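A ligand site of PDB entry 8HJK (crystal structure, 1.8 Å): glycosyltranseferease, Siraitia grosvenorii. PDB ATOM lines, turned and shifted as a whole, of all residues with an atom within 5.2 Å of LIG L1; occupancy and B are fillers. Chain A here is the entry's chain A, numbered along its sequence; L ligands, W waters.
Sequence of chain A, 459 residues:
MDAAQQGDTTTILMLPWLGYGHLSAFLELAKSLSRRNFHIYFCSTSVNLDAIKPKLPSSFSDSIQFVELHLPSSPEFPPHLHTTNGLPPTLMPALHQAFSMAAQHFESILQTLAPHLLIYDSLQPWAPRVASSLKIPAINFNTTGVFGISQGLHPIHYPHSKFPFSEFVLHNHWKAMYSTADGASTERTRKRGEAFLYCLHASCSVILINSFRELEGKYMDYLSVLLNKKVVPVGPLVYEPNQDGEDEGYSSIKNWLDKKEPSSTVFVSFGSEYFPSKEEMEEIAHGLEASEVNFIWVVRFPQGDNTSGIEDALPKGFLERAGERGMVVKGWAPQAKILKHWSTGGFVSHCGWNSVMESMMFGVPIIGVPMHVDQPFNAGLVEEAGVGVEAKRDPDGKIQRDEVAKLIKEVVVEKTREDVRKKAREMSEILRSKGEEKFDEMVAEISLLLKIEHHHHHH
The backbone NH (N) of Ser 272 lies within hydrogen-bond range of an oxygen (O11) of LIG L1, at 2.8 Å.
An oxygen (O11) of LIG L1 sits at hydrogen-bond distance from the side-chain hydroxyl (OG) of Ser 272 (2.5 Å).
An oxygen (O5) of LIG L1 sits at hydrogen-bond distance from the side-chain carboxylate (OE1) of Glu 358 (2.5 Å).
The backbone NH (N) of Ser 355 lies within hydrogen-bond range of an oxygen (O8) of LIG L1 (2.9 Å).
The side-chain hydroxyl (OG) of Ser 355 is in hydrogen-bond range of an oxygen (O8) of LIG L1 (2.7 Å).
The backbone NH (N) of Asn 354 lies within hydrogen-bond range of an oxygen (O7) of LIG L1 (2.9 Å).
The side-chain amide nitrogen (ND2) of Asn 354 is in hydrogen-bond range of an oxygen (O7) of LIG L1 (2.8 Å).
O2 of LIG L1 sits at hydrogen-bond distance from N of Ala 333, at 2.9 Å.
The backbone carbonyl oxygen (O) of Ala 333 sits at hydrogen-bond distance from a nitrogen (N2) of LIG L1.
NE2 of His 350 is in hydrogen-bond range of O12 of LIG L1.
An oxygen (O3) of LIG L1 lies close to the side-chain amide nitrogen (NE2) of Gln 335 (3.2 Å).
O1 of LIG L1 is in hydrogen-bond range of NE1 of Trp 332 (3.4 Å).
O7 of LIG L1 is in hydrogen-bond range of N of Trp 353 (3.4 Å).
OE2 of Glu 273 lies within hydrogen-bond range of O11 of LG2 L2 (2.7 Å).
A ring nitrogen (NE2) of His 22 sits at hydrogen-bond distance from an oxygen (O13) of LG2 L2, 3.1 Å away.
NE2 of Gln 335 lies within hydrogen-bond range of OE2 of Glu 358, 2.8 Å away.
OG of Ser 355 sits at hydrogen-bond distance from NE2 of Gln 335.
O of Gly 21 sits close to ND2 of Asn 354.
N of Gly 352 sits close to ND1 of His 350 (3.4 Å).
N of His 350 lies within hydrogen-bond range of O of Ser 269 (3.2 Å).
The side-chain hydroxyl of Ser 269 is in hydrogen-bond range of the backbone NH of Gly 271 (3.1 Å).
Residues that only touch LIG L1: Tyr 20, Gly 21, Ser 269, Gly 271, Glu 273, Val 298 and Gly 352.
Hydrophobic or aromatic side chains that line LIG L1: Tyr 20, Val 298, Trp 332, Ala 333 and His 350.
Along chain A the residues within 4 Å of LIG L1 span positions 20 to 358.
Water W5 bridges O12 of LIG L1 (2.4 Å) and OE2 of Glu 273 (3.1 Å).
Water W3 lies within hydrogen-bond range of O12 of LIG L1 (2.5 Å), N of Glu 273 (2.9 Å), O of Phe 270 (3.0 Å), N of Ser 272 (3.4 Å) and NE2 of His 350 (3.5 Å).
Water W2 lies within hydrogen-bond range of an oxygen (O10) of LIG L1 (2.6 Å), the side-chain carboxylate of Glu 273 (2.8 Å), the backbone NH of Gly 21 (3.0 Å) and the backbone NH of Tyr 20 (3.5 Å).
Water W6 lies within hydrogen-bond range of O1 of LIG L1, NE1 of Trp 332 and O of Ala 333.
Water W4 lies within hydrogen-bond range of the side-chain amide oxygen of Gln 335, the side-chain hydroxyl of Ser 269, the side-chain hydroxyl of Ser 355 and the backbone NH of Gly 271.
Water W1 lies within hydrogen-bond range of NE2 of Gln 375 (2.9 Å), O12 of LIG L1 (3.5 Å) and O of Glu 273 (3.5 Å).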
ATOM      1  N   TYR A  20     -10.509  20.427   2.177  1.00  0.00           N
ATOM      2  CA  TYR A  20      -9.332  19.948   1.421  1.00  0.00           C
ATOM      3  C   TYR A  20      -9.754  19.184   0.155  1.00  0.00           C
ATOM      4  O   TYR A  20      -9.110  19.309  -0.857  1.00  0.00           O
ATOM      5  CB  TYR A  20      -8.478  19.101   2.353  1.00  0.00           C
ATOM      6  CG  TYR A  20      -7.202  18.592   1.732  1.00  0.00           C
ATOM      7  CD1 TYR A  20      -6.069  19.392   1.683  1.00  0.00           C
ATOM      8  CD2 TYR A  20      -7.115  17.321   1.186  1.00  0.00           C
ATOM      9  CE1 TYR A  20      -4.897  18.946   1.107  1.00  0.00           C
ATOM     10  CE2 TYR A  20      -5.946  16.861   0.614  1.00  0.00           C
ATOM     11  CZ  TYR A  20      -4.832  17.675   0.569  1.00  0.00           C
ATOM     12  OH  TYR A  20      -3.678  17.224   0.014  1.00  0.00           O
ATOM     13  N   GLY A  21     -10.812  18.390   0.250  1.00  0.00           N
ATOM     14  CA  GLY A  21     -11.304  17.664  -0.929  1.00  0.00           C
ATOM     15  C   GLY A  21     -11.764  18.604  -2.026  1.00  0.00           C
ATOM     16  O   GLY A  21     -11.451  18.386  -3.183  1.00  0.00           O
ATOM     17  N   HIS A  22     -12.495  19.645  -1.634  1.00  0.00           N
ATOM     18  CA  HIS A  22     -12.960  20.661  -2.600  1.00  0.00           C
ATOM     19  C   HIS A  22     -11.776  21.414  -3.194  1.00  0.00           C
ATOM     20  O   HIS A  22     -11.736  21.577  -4.401  1.00  0.00           O
ATOM     21  CB  HIS A  22     -13.957  21.580  -1.894  1.00  0.00           C
ATOM     22  CG  HIS A  22     -15.198  20.906  -1.418  1.00  0.00           C
ATOM     23  ND1 HIS A  22     -16.445  21.218  -1.918  1.00  0.00           N
ATOM     24  CD2 HIS A  22     -15.399  19.949  -0.489  1.00  0.00           C
ATOM     25  CE1 HIS A  22     -17.351  20.481  -1.321  1.00  0.00           C
ATOM     26  NE2 HIS A  22     -16.738  19.696  -0.450  1.00  0.00           N
ATOM     27  N   PHE A 267      -6.499  -0.331   3.461  1.00  0.00           N
ATOM     28  CA  PHE A 267      -6.298   1.008   3.992  1.00  0.00           C
ATOM     29  C   PHE A 267      -7.612   1.465   4.618  1.00  0.00           C
ATOM     30  O   PHE A 267      -8.683   1.158   4.099  1.00  0.00           O
ATOM     31  CB  PHE A 267      -5.876   1.939   2.843  1.00  0.00           C
ATOM     32  CG  PHE A 267      -5.632   3.353   3.265  1.00  0.00           C
ATOM     33  CD1 PHE A 267      -4.667   3.633   4.213  1.00  0.00           C
ATOM     34  CD2 PHE A 267      -6.340   4.401   2.697  1.00  0.00           C
ATOM     35  CE1 PHE A 267      -4.424   4.919   4.638  1.00  0.00           C
ATOM     36  CE2 PHE A 267      -6.096   5.718   3.101  1.00  0.00           C
ATOM     37  CZ  PHE A 267      -5.125   5.976   4.078  1.00  0.00           C
ATOM     38  N   SER A 269      -9.549   4.847   6.178  1.00  0.00           N
ATOM     39  CA  SER A 269      -9.487   6.297   6.340  1.00  0.00           C
ATOM     40  C   SER A 269     -10.882   6.901   6.299  1.00  0.00           C
ATOM     41  O   SER A 269     -11.759   6.427   5.578  1.00  0.00           O
ATOM     42  CB  SER A 269      -8.640   6.990   5.264  1.00  0.00           C
ATOM     43  OG  SER A 269      -8.807   8.402   5.349  1.00  0.00           O
ATOM     44  N   PHE A 270     -11.062   7.977   7.059  1.00  0.00           N
ATOM     45  CA  PHE A 270     -12.336   8.688   7.074  1.00  0.00           C
ATOM     46  C   PHE A 270     -12.179  10.134   6.626  1.00  0.00           C
ATOM     47  O   PHE A 270     -12.985  11.003   6.979  1.00  0.00           O
ATOM     48  CB  PHE A 270     -12.968   8.543   8.457  1.00  0.00           C
ATOM     49  CG  PHE A 270     -13.201   7.101   8.824  1.00  0.00           C
ATOM     50  CD1 PHE A 270     -14.289   6.408   8.305  1.00  0.00           C
ATOM     51  CD2 PHE A 270     -12.274   6.418   9.595  1.00  0.00           C
ATOM     52  CE1 PHE A 270     -14.482   5.054   8.600  1.00  0.00           C
ATOM     53  CE2 PHE A 270     -12.467   5.068   9.899  1.00  0.00           C
ATOM     54  CZ  PHE A 270     -13.572   4.387   9.406  1.00  0.00           C
ATOM     55  N   GLY A 271     -11.174  10.397   5.803  1.00  0.00           N
ATOM     56  CA  GLY A 271     -11.072  11.659   5.097  1.00  0.00           C
ATOM     57  C   GLY A 271     -10.434  12.746   5.932  1.00  0.00           C
ATOM     58  O   GLY A 271      -9.758  12.498   6.933  1.00  0.00           O
ATOM     59  N   SER A 272     -10.669  14.007   5.512  1.00  0.00           N
ATOM     60  CA  SER A 272      -9.997  15.162   6.080  1.00  0.00           C
ATOM     61  C   SER A 272     -10.844  15.939   7.092  1.00  0.00           C
ATOM     62  O   SER A 272     -10.294  16.793   7.792  1.00  0.00           O
ATOM     63  CB  SER A 272      -9.541  16.097   4.943  1.00  0.00           C
ATOM     64  OG  SER A 272     -10.667  16.721   4.339  1.00  0.00           O
ATOM     65  N   GLU A 273     -12.132  15.663   7.208  1.00  0.00           N
ATOM     66  CA  GLU A 273     -12.987  16.457   8.086  1.00  0.00           C
ATOM     67  C   GLU A 273     -13.985  15.572   8.794  1.00  0.00           C
ATOM     68  O   GLU A 273     -15.177  15.908   8.886  1.00  0.00           O
ATOM     69  CB  GLU A 273     -13.675  17.568   7.294  1.00  0.00           C
ATOM     70  CG  GLU A 273     -14.281  17.087   5.997  1.00  0.00           C
ATOM     71  CD  GLU A 273     -14.944  18.207   5.182  1.00  0.00           C
ATOM     72  OE1 GLU A 273     -14.221  19.045   4.578  1.00  0.00           O
ATOM     73  OE2 GLU A 273     -16.185  18.257   5.162  1.00  0.00           O
ATOM     74  N   VAL A 298      -5.435   5.259   9.410  1.00  0.00           N
ATOM     75  CA  VAL A 298      -5.073   6.654   9.741  1.00  0.00           C
ATOM     76  C   VAL A 298      -6.023   7.107  10.832  1.00  0.00           C
ATOM     77  O   VAL A 298      -7.223   7.076  10.609  1.00  0.00           O
ATOM     78  CB  VAL A 298      -5.152   7.629   8.551  1.00  0.00           C
ATOM     79  CG1 VAL A 298      -4.488   8.954   8.854  1.00  0.00           C
ATOM     80  CG2 VAL A 298      -4.594   7.001   7.294  1.00  0.00           C
ATOM     81  N   GLY A 331      -2.434  11.174  12.065  1.00  0.00           N
ATOM     82  CA  GLY A 331      -2.515  12.459  11.350  1.00  0.00           C
ATOM     83  C   GLY A 331      -2.893  12.335   9.907  1.00  0.00           C
ATOM     84  O   GLY A 331      -4.050  12.548   9.578  1.00  0.00           O
ATOM     85  N   TRP A 332      -1.894  12.152   9.075  1.00  0.00           N
ATOM     86  CA  TRP A 332      -2.164  12.138   7.622  1.00  0.00           C
ATOM     87  C   TRP A 332      -1.354  11.011   7.010  1.00  0.00           C
ATOM     88  O   TRP A 332      -0.218  10.800   7.444  1.00  0.00           O
ATOM     89  CB  TRP A 332      -1.786  13.479   7.014  1.00  0.00           C
ATOM     90  CG  TRP A 332      -2.322  13.795   5.657  1.00  0.00           C
ATOM     91  CD1 TRP A 332      -1.651  13.779   4.474  1.00  0.00           C
ATOM     92  CD2 TRP A 332      -3.651  14.252   5.366  1.00  0.00           C
ATOM     93  NE1 TRP A 332      -2.467  14.167   3.455  1.00  0.00           N
ATOM     94  CE2 TRP A 332      -3.708  14.464   3.974  1.00  0.00           C
ATOM     95  CE3 TRP A 332      -4.792  14.491   6.137  1.00  0.00           C
ATOM     96  CZ2 TRP A 332      -4.869  14.909   3.337  1.00  0.00           C
ATOM     97  CZ3 TRP A 332      -5.937  14.912   5.509  1.00  0.00           C
ATOM     98  CH2 TRP A 332      -5.967  15.123   4.130  1.00  0.00           C
ATOM     99  N   ALA A 333      -1.932  10.358   6.033  1.00  0.00           N
ATOM    100  CA  ALA A 333      -1.224   9.267   5.370  1.00  0.00           C
ATOM    101  C   ALA A 333      -1.122   9.520   3.868  1.00  0.00           C
ATOM    102  O   ALA A 333      -1.898  10.311   3.356  1.00  0.00           O
ATOM    103  CB  ALA A 333      -1.911   7.970   5.641  1.00  0.00           C
ATOM    104  N   PRO A 334      -0.147   8.916   3.153  1.00  0.00           N
ATOM    105  CA  PRO A 334      -0.109   9.031   1.676  1.00  0.00           C
ATOM    106  C   PRO A 334      -1.123   8.096   1.036  1.00  0.00           C
ATOM    107  O   PRO A 334      -0.805   6.987   0.554  1.00  0.00           O
ATOM    108  CB  PRO A 334       1.341   8.662   1.347  1.00  0.00           C
ATOM    109  CG  PRO A 334       1.723   7.699   2.458  1.00  0.00           C
ATOM    110  CD  PRO A 334       1.010   8.172   3.696  1.00  0.00           C
ATOM    111  N   GLN A 335      -2.373   8.556   1.027  1.00  0.00           N
ATOM    112  CA  GLN A 335      -3.490   7.711   0.625  1.00  0.00           C
ATOM    113  C   GLN A 335      -3.309   7.167  -0.786  1.00  0.00           C
ATOM    114  O   GLN A 335      -3.473   5.970  -1.036  1.00  0.00           O
ATOM    115  CB  GLN A 335      -4.810   8.480   0.733  1.00  0.00           C
ATOM    116  CG  GLN A 335      -6.001   7.810   0.038  1.00  0.00           C
ATOM    117  CD  GLN A 335      -7.354   8.306   0.573  1.00  0.00           C
ATOM    118  OE1 GLN A 335      -7.496   8.585   1.773  1.00  0.00           O
ATOM    119  NE2 GLN A 335      -8.345   8.422  -0.307  1.00  0.00           N
ATOM    120  N   ALA A 336      -2.975   8.040  -1.739  1.00  0.00           N
ATOM    121  CA  ALA A 336      -2.856   7.584  -3.111  1.00  0.00           C
ATOM    122  C   ALA A 336      -1.753   6.546  -3.254  1.00  0.00           C
ATOM    123  O   ALA A 336      -1.928   5.511  -3.905  1.00  0.00           O
ATOM    124  CB  ALA A 336      -2.616   8.761  -4.042  1.00  0.00           C
ATOM    125  N   HIS A 350     -14.737   6.210   4.327  1.00  0.00           N
ATOM    126  CA  HIS A 350     -15.954   6.952   4.601  1.00  0.00           C
ATOM    127  C   HIS A 350     -16.735   7.299   3.333  1.00  0.00           C
ATOM    128  O   HIS A 350     -17.830   7.852   3.471  1.00  0.00           O
ATOM    129  CB  HIS A 350     -15.641   8.221   5.400  1.00  0.00           C
ATOM    130  CG  HIS A 350     -15.033   9.318   4.588  1.00  0.00           C
ATOM    131  ND1 HIS A 350     -13.963   9.116   3.745  1.00  0.00           N
ATOM    132  CD2 HIS A 350     -15.313  10.651   4.544  1.00  0.00           C
ATOM    133  CE1 HIS A 350     -13.617  10.277   3.190  1.00  0.00           C
ATOM    134  NE2 HIS A 350     -14.422  11.211   3.669  1.00  0.00           N
ATOM    135  N   GLY A 352     -16.061   9.545   1.065  1.00  0.00           N
ATOM    136  CA  GLY A 352     -15.883  10.865   0.461  1.00  0.00           C
ATOM    137  C   GLY A 352     -15.599  10.723  -1.023  1.00  0.00           C
ATOM    138  O   GLY A 352     -14.986   9.757  -1.472  1.00  0.00           O
ATOM    139  N   TRP A 353     -16.027  11.728  -1.801  1.00  0.00           N
ATOM    140  CA  TRP A 353     -16.028  11.555  -3.252  1.00  0.00           C
ATOM    141  C   TRP A 353     -14.626  11.423  -3.830  1.00  0.00           C
ATOM    142  O   TRP A 353     -14.399  10.598  -4.719  1.00  0.00           O
ATOM    143  CB  TRP A 353     -16.745  12.720  -3.927  1.00  0.00           C
ATOM    144  CG  TRP A 353     -17.003  12.512  -5.404  1.00  0.00           C
ATOM    145  CD1 TRP A 353     -16.408  13.194  -6.451  1.00  0.00           C
ATOM    146  CD2 TRP A 353     -17.920  11.586  -5.998  1.00  0.00           C
ATOM    147  NE1 TRP A 353     -16.901  12.729  -7.650  1.00  0.00           N
ATOM    148  CE2 TRP A 353     -17.832  11.756  -7.396  1.00  0.00           C
ATOM    149  CE3 TRP A 353     -18.801  10.635  -5.492  1.00  0.00           C
ATOM    150  CZ2 TRP A 353     -18.614  10.996  -8.285  1.00  0.00           C
ATOM    151  CZ3 TRP A 353     -19.555   9.891  -6.363  1.00  0.00           C
ATOM    152  CH2 TRP A 353     -19.459  10.069  -7.753  1.00  0.00           C
ATOM    153  N   ASN A 354     -13.660  12.237  -3.374  1.00  0.00           N
ATOM    154  CA  ASN A 354     -12.322  12.076  -3.946  1.00  0.00           C
ATOM    155  C   ASN A 354     -11.746  10.705  -3.622  1.00  0.00           C
ATOM    156  O   ASN A 354     -11.033  10.126  -4.460  1.00  0.00           O
ATOM    157  CB  ASN A 354     -11.393  13.169  -3.434  1.00  0.00           C
ATOM    158  CG  ASN A 354     -11.872  14.541  -3.825  1.00  0.00           C
ATOM    159  OD1 ASN A 354     -11.876  14.890  -5.007  1.00  0.00           O
ATOM    160  ND2 ASN A 354     -12.324  15.306  -2.855  1.00  0.00           N
ATOM    161  N   SER A 355     -12.036  10.181  -2.430  1.00  0.00           N
ATOM    162  CA  SER A 355     -11.523   8.868  -2.046  1.00  0.00           C
ATOM    163  C   SER A 355     -12.151   7.776  -2.911  1.00  0.00           C
ATOM    164  O   SER A 355     -11.478   6.796  -3.276  1.00  0.00           O
ATOM    165  CB  SER A 355     -11.852   8.628  -0.565  1.00  0.00           C
ATOM    166  OG  SER A 355     -10.989   9.398   0.273  1.00  0.00           O
ATOM    167  N   VAL A 356     -13.436   7.897  -3.216  1.00  0.00           N
ATOM    168  CA  VAL A 356     -14.085   6.945  -4.111  1.00  0.00           C
ATOM    169  C   VAL A 356     -13.451   7.008  -5.506  1.00  0.00           C
ATOM    170  O   VAL A 356     -13.118   5.979  -6.101  1.00  0.00           O
ATOM    171  CB  VAL A 356     -15.605   7.199  -4.161  1.00  0.00           C
ATOM    172  CG1 VAL A 356     -16.257   6.371  -5.250  1.00  0.00           C
ATOM    173  CG2 VAL A 356     -16.243   6.889  -2.794  1.00  0.00           C
ATOM    174  N   GLU A 358     -10.499   8.023  -6.347  1.00  0.00           N
ATOM    175  CA  GLU A 358      -9.126   7.476  -6.286  1.00  0.00           C
ATOM    176  C   GLU A 358      -9.173   5.951  -6.281  1.00  0.00           C
ATOM    177  O   GLU A 358      -8.440   5.343  -7.033  1.00  0.00           O
ATOM    178  CB  GLU A 358      -8.458   8.001  -5.022  1.00  0.00           C
ATOM    179  CG  GLU A 358      -8.029   9.446  -5.121  1.00  0.00           C
ATOM    180  CD  GLU A 358      -7.767  10.137  -3.796  1.00  0.00           C
ATOM    181  OE1 GLU A 358      -7.683  11.367  -3.766  1.00  0.00           O
ATOM    182  OE2 GLU A 358      -7.659   9.430  -2.786  1.00  0.00           O
ATOM    183  N   GLN A 375     -21.853  11.171   1.729  1.00  0.00           N
ATOM    184  CA  GLN A 375     -21.231   9.829   1.854  1.00  0.00           C
ATOM    185  C   GLN A 375     -22.247   8.671   1.743  1.00  0.00           C
ATOM    186  O   GLN A 375     -21.952   7.741   1.013  1.00  0.00           O
ATOM    187  CB  GLN A 375     -20.334   9.779   3.087  1.00  0.00           C
ATOM    188  CG  GLN A 375     -19.195  10.777   3.041  1.00  0.00           C
ATOM    189  CD  GLN A 375     -18.820  11.248   4.421  1.00  0.00           C
ATOM    190  OE1 GLN A 375     -19.061  10.558   5.410  1.00  0.00           O
ATOM    191  NE2 GLN A 375     -18.238  12.421   4.496  1.00  0.00           N
HETATM  192  N1  LIG L   1      -6.305  12.138   2.181  1.00  0.00           N
HETATM  193  C1  LIG L   1      -4.966  11.841   2.277  1.00  0.00           C
HETATM  194  N2  LIG L   1      -4.538  11.315   3.467  1.00  0.00           N
HETATM  195  C2  LIG L   1      -5.326  11.062   4.568  1.00  0.00           C
HETATM  196  C3  LIG L   1      -6.711  11.379   4.409  1.00  0.00           C
HETATM  197  C4  LIG L   1      -7.171  11.902   3.239  1.00  0.00           C
HETATM  198  O1  LIG L   1      -4.181  12.048   1.351  1.00  0.00           O
HETATM  199  O2  LIG L   1      -4.810  10.581   5.589  1.00  0.00           O
HETATM  200  C5  LIG L   1      -6.810  12.711   0.925  1.00  0.00           C
HETATM  201  C6  LIG L   1      -7.567  11.653   0.050  1.00  0.00           C
HETATM  202  O3  LIG L   1      -6.634  11.052  -0.839  1.00  0.00           O
HETATM  203  C7  LIG L   1      -8.528  12.520  -0.715  1.00  0.00           C
HETATM  204  C8  LIG L   1      -8.834  13.660   0.258  1.00  0.00           C
HETATM  205  O4  LIG L   1      -7.774  13.689   1.249  1.00  0.00           O
HETATM  206  O5  LIG L   1      -7.864  13.046  -1.882  1.00  0.00           O
HETATM  207  C9  LIG L   1     -10.128  13.392   0.966  1.00  0.00           C
HETATM  208  O6  LIG L   1     -11.147  13.885   0.141  1.00  0.00           O
HETATM  209  P1  LIG L   1     -12.591  13.119   0.177  1.00  0.00           P
HETATM  210  O7  LIG L   1     -13.494  13.736  -0.856  1.00  0.00           O
HETATM  211  O8  LIG L   1     -12.422  11.640  -0.011  1.00  0.00           O
HETATM  212  O9  LIG L   1     -13.254  13.293   1.666  1.00  0.00           O
HETATM  213  P2  LIG L   1     -13.379  14.600   2.644  1.00  0.00           P
HETATM  214  O10 LIG L   1     -13.857  15.767   1.815  1.00  0.00           O
HETATM  215  O11 LIG L   1     -12.039  14.903   3.258  1.00  0.00           O
HETATM  216  O12 LIG L   1     -14.413  14.272   3.702  1.00  0.00           O
HETATM  217  O1  LG2 L   2     -33.649  22.451  -0.842  1.00  0.00           O
HETATM  218  O2  LG2 L   2     -19.381  21.463   5.619  1.00  0.00           O
HETATM  219  O3  LG2 L   2     -43.113  21.730  -1.069  1.00  0.00           O
HETATM  220  O4  LG2 L   2     -43.615  19.229   0.664  1.00  0.00           O
HETATM  221  C1  LG2 L   2     -28.962  16.974   1.258  1.00  0.00           C
HETATM  222  C2  LG2 L   2     -29.342  17.220  -0.222  1.00  0.00           C
HETATM  223  C3  LG2 L   2     -27.515  16.491   1.440  1.00  0.00           C
HETATM  224  C4  LG2 L   2     -26.393  17.137   0.475  1.00  0.00           C
HETATM  225  C5  LG2 L   2     -30.657  18.022  -0.104  1.00  0.00           C
HETATM  226  C6  LG2 L   2     -28.265  17.043  -1.296  1.00  0.00           C
HETATM  227  C7  LG2 L   2     -30.324  16.415   1.812  1.00  0.00           C
HETATM  228  C8  LG2 L   2     -26.929  17.592  -0.921  1.00  0.00           C
HETATM  229  C9  LG2 L   2     -25.559  18.311   1.090  1.00  0.00           C
HETATM  230  C10 LG2 L   2     -31.465  16.989   0.767  1.00  0.00           C
HETATM  231  C11 LG2 L   2     -27.118  16.417   2.965  1.00  0.00           C
HETATM  232  C12 LG2 L   2     -29.064  18.413   1.860  1.00  0.00           C
HETATM  233  C13 LG2 L   2     -29.905  15.770  -0.312  1.00  0.00           C
HETATM  234  C14 LG2 L   2     -31.378  18.544  -1.271  1.00  0.00           C
HETATM  235  C15 LG2 L   2     -25.267  18.245   2.658  1.00  0.00           C
HETATM  236  C16 LG2 L   2     -25.405  16.002   0.199  1.00  0.00           C
HETATM  237  C17 LG2 L   2     -24.261  18.565   0.344  1.00  0.00           C
HETATM  238  C18 LG2 L   2     -26.332  17.664   3.561  1.00  0.00           C
HETATM  239  C19 LG2 L   2     -24.859  19.700   2.992  1.00  0.00           C
HETATM  240  C20 LG2 L   2     -23.645  19.837   0.726  1.00  0.00           C
HETATM  241  C21 LG2 L   2     -23.573  20.081   2.231  1.00  0.00           C
HETATM  242  C22 LG2 L   2     -32.821  18.712  -0.880  1.00  0.00           C
HETATM  243  C23 LG2 L   2     -31.347  17.744  -2.610  1.00  0.00           C
HETATM  244  C24 LG2 L   2     -24.647  19.804   4.515  1.00  0.00           C
HETATM  245  C25 LG2 L   2     -25.993  20.692   2.606  1.00  0.00           C
HETATM  246  C26 LG2 L   2     -33.008  20.127  -0.158  1.00  0.00           C
HETATM  247  C27 LG2 L   2     -34.519  20.404   0.019  1.00  0.00           C
HETATM  248  C28 LG2 L   2     -21.317  20.127   2.694  1.00  0.00           C
HETATM  249  C29 LG2 L   2     -34.844  21.767  -0.562  1.00  0.00           C
HETATM  250  C30 LG2 L   2     -21.014  20.626   4.112  1.00  0.00           C
HETATM  251  C31 LG2 L   2     -19.593  20.950   4.266  1.00  0.00           C
HETATM  252  C32 LG2 L   2     -35.676  22.613   0.438  1.00  0.00           C
HETATM  253  C33 LG2 L   2     -35.664  21.584  -1.864  1.00  0.00           C
HETATM  254  C34 LG2 L   2     -19.273  18.768   3.053  1.00  0.00           C
HETATM  255  C35 LG2 L   2     -18.766  19.744   4.121  1.00  0.00           C
HETATM  256  C36 LG2 L   2     -35.450  19.183   1.833  1.00  0.00           C
HETATM  257  C37 LG2 L   2     -34.792  18.701   3.141  1.00  0.00           C
HETATM  258  C38 LG2 L   2     -18.047  18.277   2.337  1.00  0.00           C
HETATM  259  C39 LG2 L   2     -35.498  19.003   4.421  1.00  0.00           C
HETATM  260  C40 LG2 L   2     -37.156  20.315   3.072  1.00  0.00           C
HETATM  261  C41 LG2 L   2     -36.871  19.550   4.361  1.00  0.00           C
HETATM  262  C42 LG2 L   2     -38.618  20.745   3.037  1.00  0.00           C
HETATM  263  C43 LG2 L   2     -35.470  16.610   2.252  1.00  0.00           C
HETATM  264  C44 LG2 L   2     -34.784  15.452   1.493  1.00  0.00           C
HETATM  265  C45 LG2 L   2     -36.243  14.820   3.697  1.00  0.00           C
HETATM  266  C46 LG2 L   2     -36.085  13.725   2.645  1.00  0.00           C
HETATM  267  C47 LG2 L   2     -39.793  21.975   1.390  1.00  0.00           C
HETATM  268  C48 LG2 L   2     -39.608  22.348  -0.086  1.00  0.00           C
HETATM  269  C49 LG2 L   2     -37.344  14.441   4.652  1.00  0.00           C
HETATM  270  C50 LG2 L   2     -40.894  22.521  -0.794  1.00  0.00           C
HETATM  271  C51 LG2 L   2     -41.800  20.771   0.724  1.00  0.00           C
HETATM  272  C52 LG2 L   2     -41.769  21.347  -0.686  1.00  0.00           C
HETATM  273  C53 LG2 L   2     -43.232  20.508   1.113  1.00  0.00           C
HETATM  274  O5  LG2 L   2     -26.094  17.209  -1.864  1.00  0.00           O
HETATM  275  O6  LG2 L   2     -22.465  19.332   2.751  1.00  0.00           O
HETATM  276  O7  LG2 L   2     -34.822  20.367   1.417  1.00  0.00           O
HETATM  277  O8  LG2 L   2     -20.203  19.369   2.088  1.00  0.00           O
HETATM  278  O9  LG2 L   2     -21.771  21.829   4.380  1.00  0.00           O
HETATM  279  O10 LG2 L   2     -36.891  19.459   1.919  1.00  0.00           O
HETATM  280  O11 LG2 L   2     -17.435  20.154   3.758  1.00  0.00           O
HETATM  281  O12 LG2 L   2     -34.545  17.257   3.063  1.00  0.00           O
HETATM  282  O13 LG2 L   2     -18.373  17.559   1.178  1.00  0.00           O
HETATM  283  O14 LG2 L   2     -34.670  19.960   5.178  1.00  0.00           O
HETATM  284  O15 LG2 L   2     -37.825  18.464   4.473  1.00  0.00           O
HETATM  285  O16 LG2 L   2     -39.031  20.843   1.662  1.00  0.00           O
HETATM  286  O17 LG2 L   2     -36.576  16.111   3.079  1.00  0.00           O
HETATM  287  O18 LG2 L   2     -34.923  13.243   0.588  1.00  0.00           O
HETATM  288  O19 LG2 L   2     -41.192  21.679   1.707  1.00  0.00           O
HETATM  289  O20 LG2 L   2     -37.352  13.059   2.465  1.00  0.00           O
HETATM  290  O21 LG2 L   2     -38.885  23.603  -0.148  1.00  0.00           O
HETATM  291  O22 LG2 L   2     -37.888  15.610   5.224  1.00  0.00           O
HETATM  292  O23 LG2 L   2     -40.607  22.765  -2.226  1.00  0.00           O
HETATM  293  O   HOH W   1     -16.680  14.093   6.314  1.00  0.00           O
HETATM  294  O   HOH W   2     -13.274  18.336   1.992  1.00  0.00           O
HETATM  295  O   HOH W   3     -13.957  13.654   6.122  1.00  0.00           O
HETATM  296  O   HOH W   4      -9.639   9.516   2.990  1.00  0.00           O
HETATM  297  O   HOH W   5     -16.539  15.477   3.862  1.00  0.00           O
HETATM  298  O   HOH W   6      -1.533  12.424   0.635  1.00  0.00           O
HETATM  299  O   HOH W   7     -15.479  15.816  -0.438  1.00  0.00           O
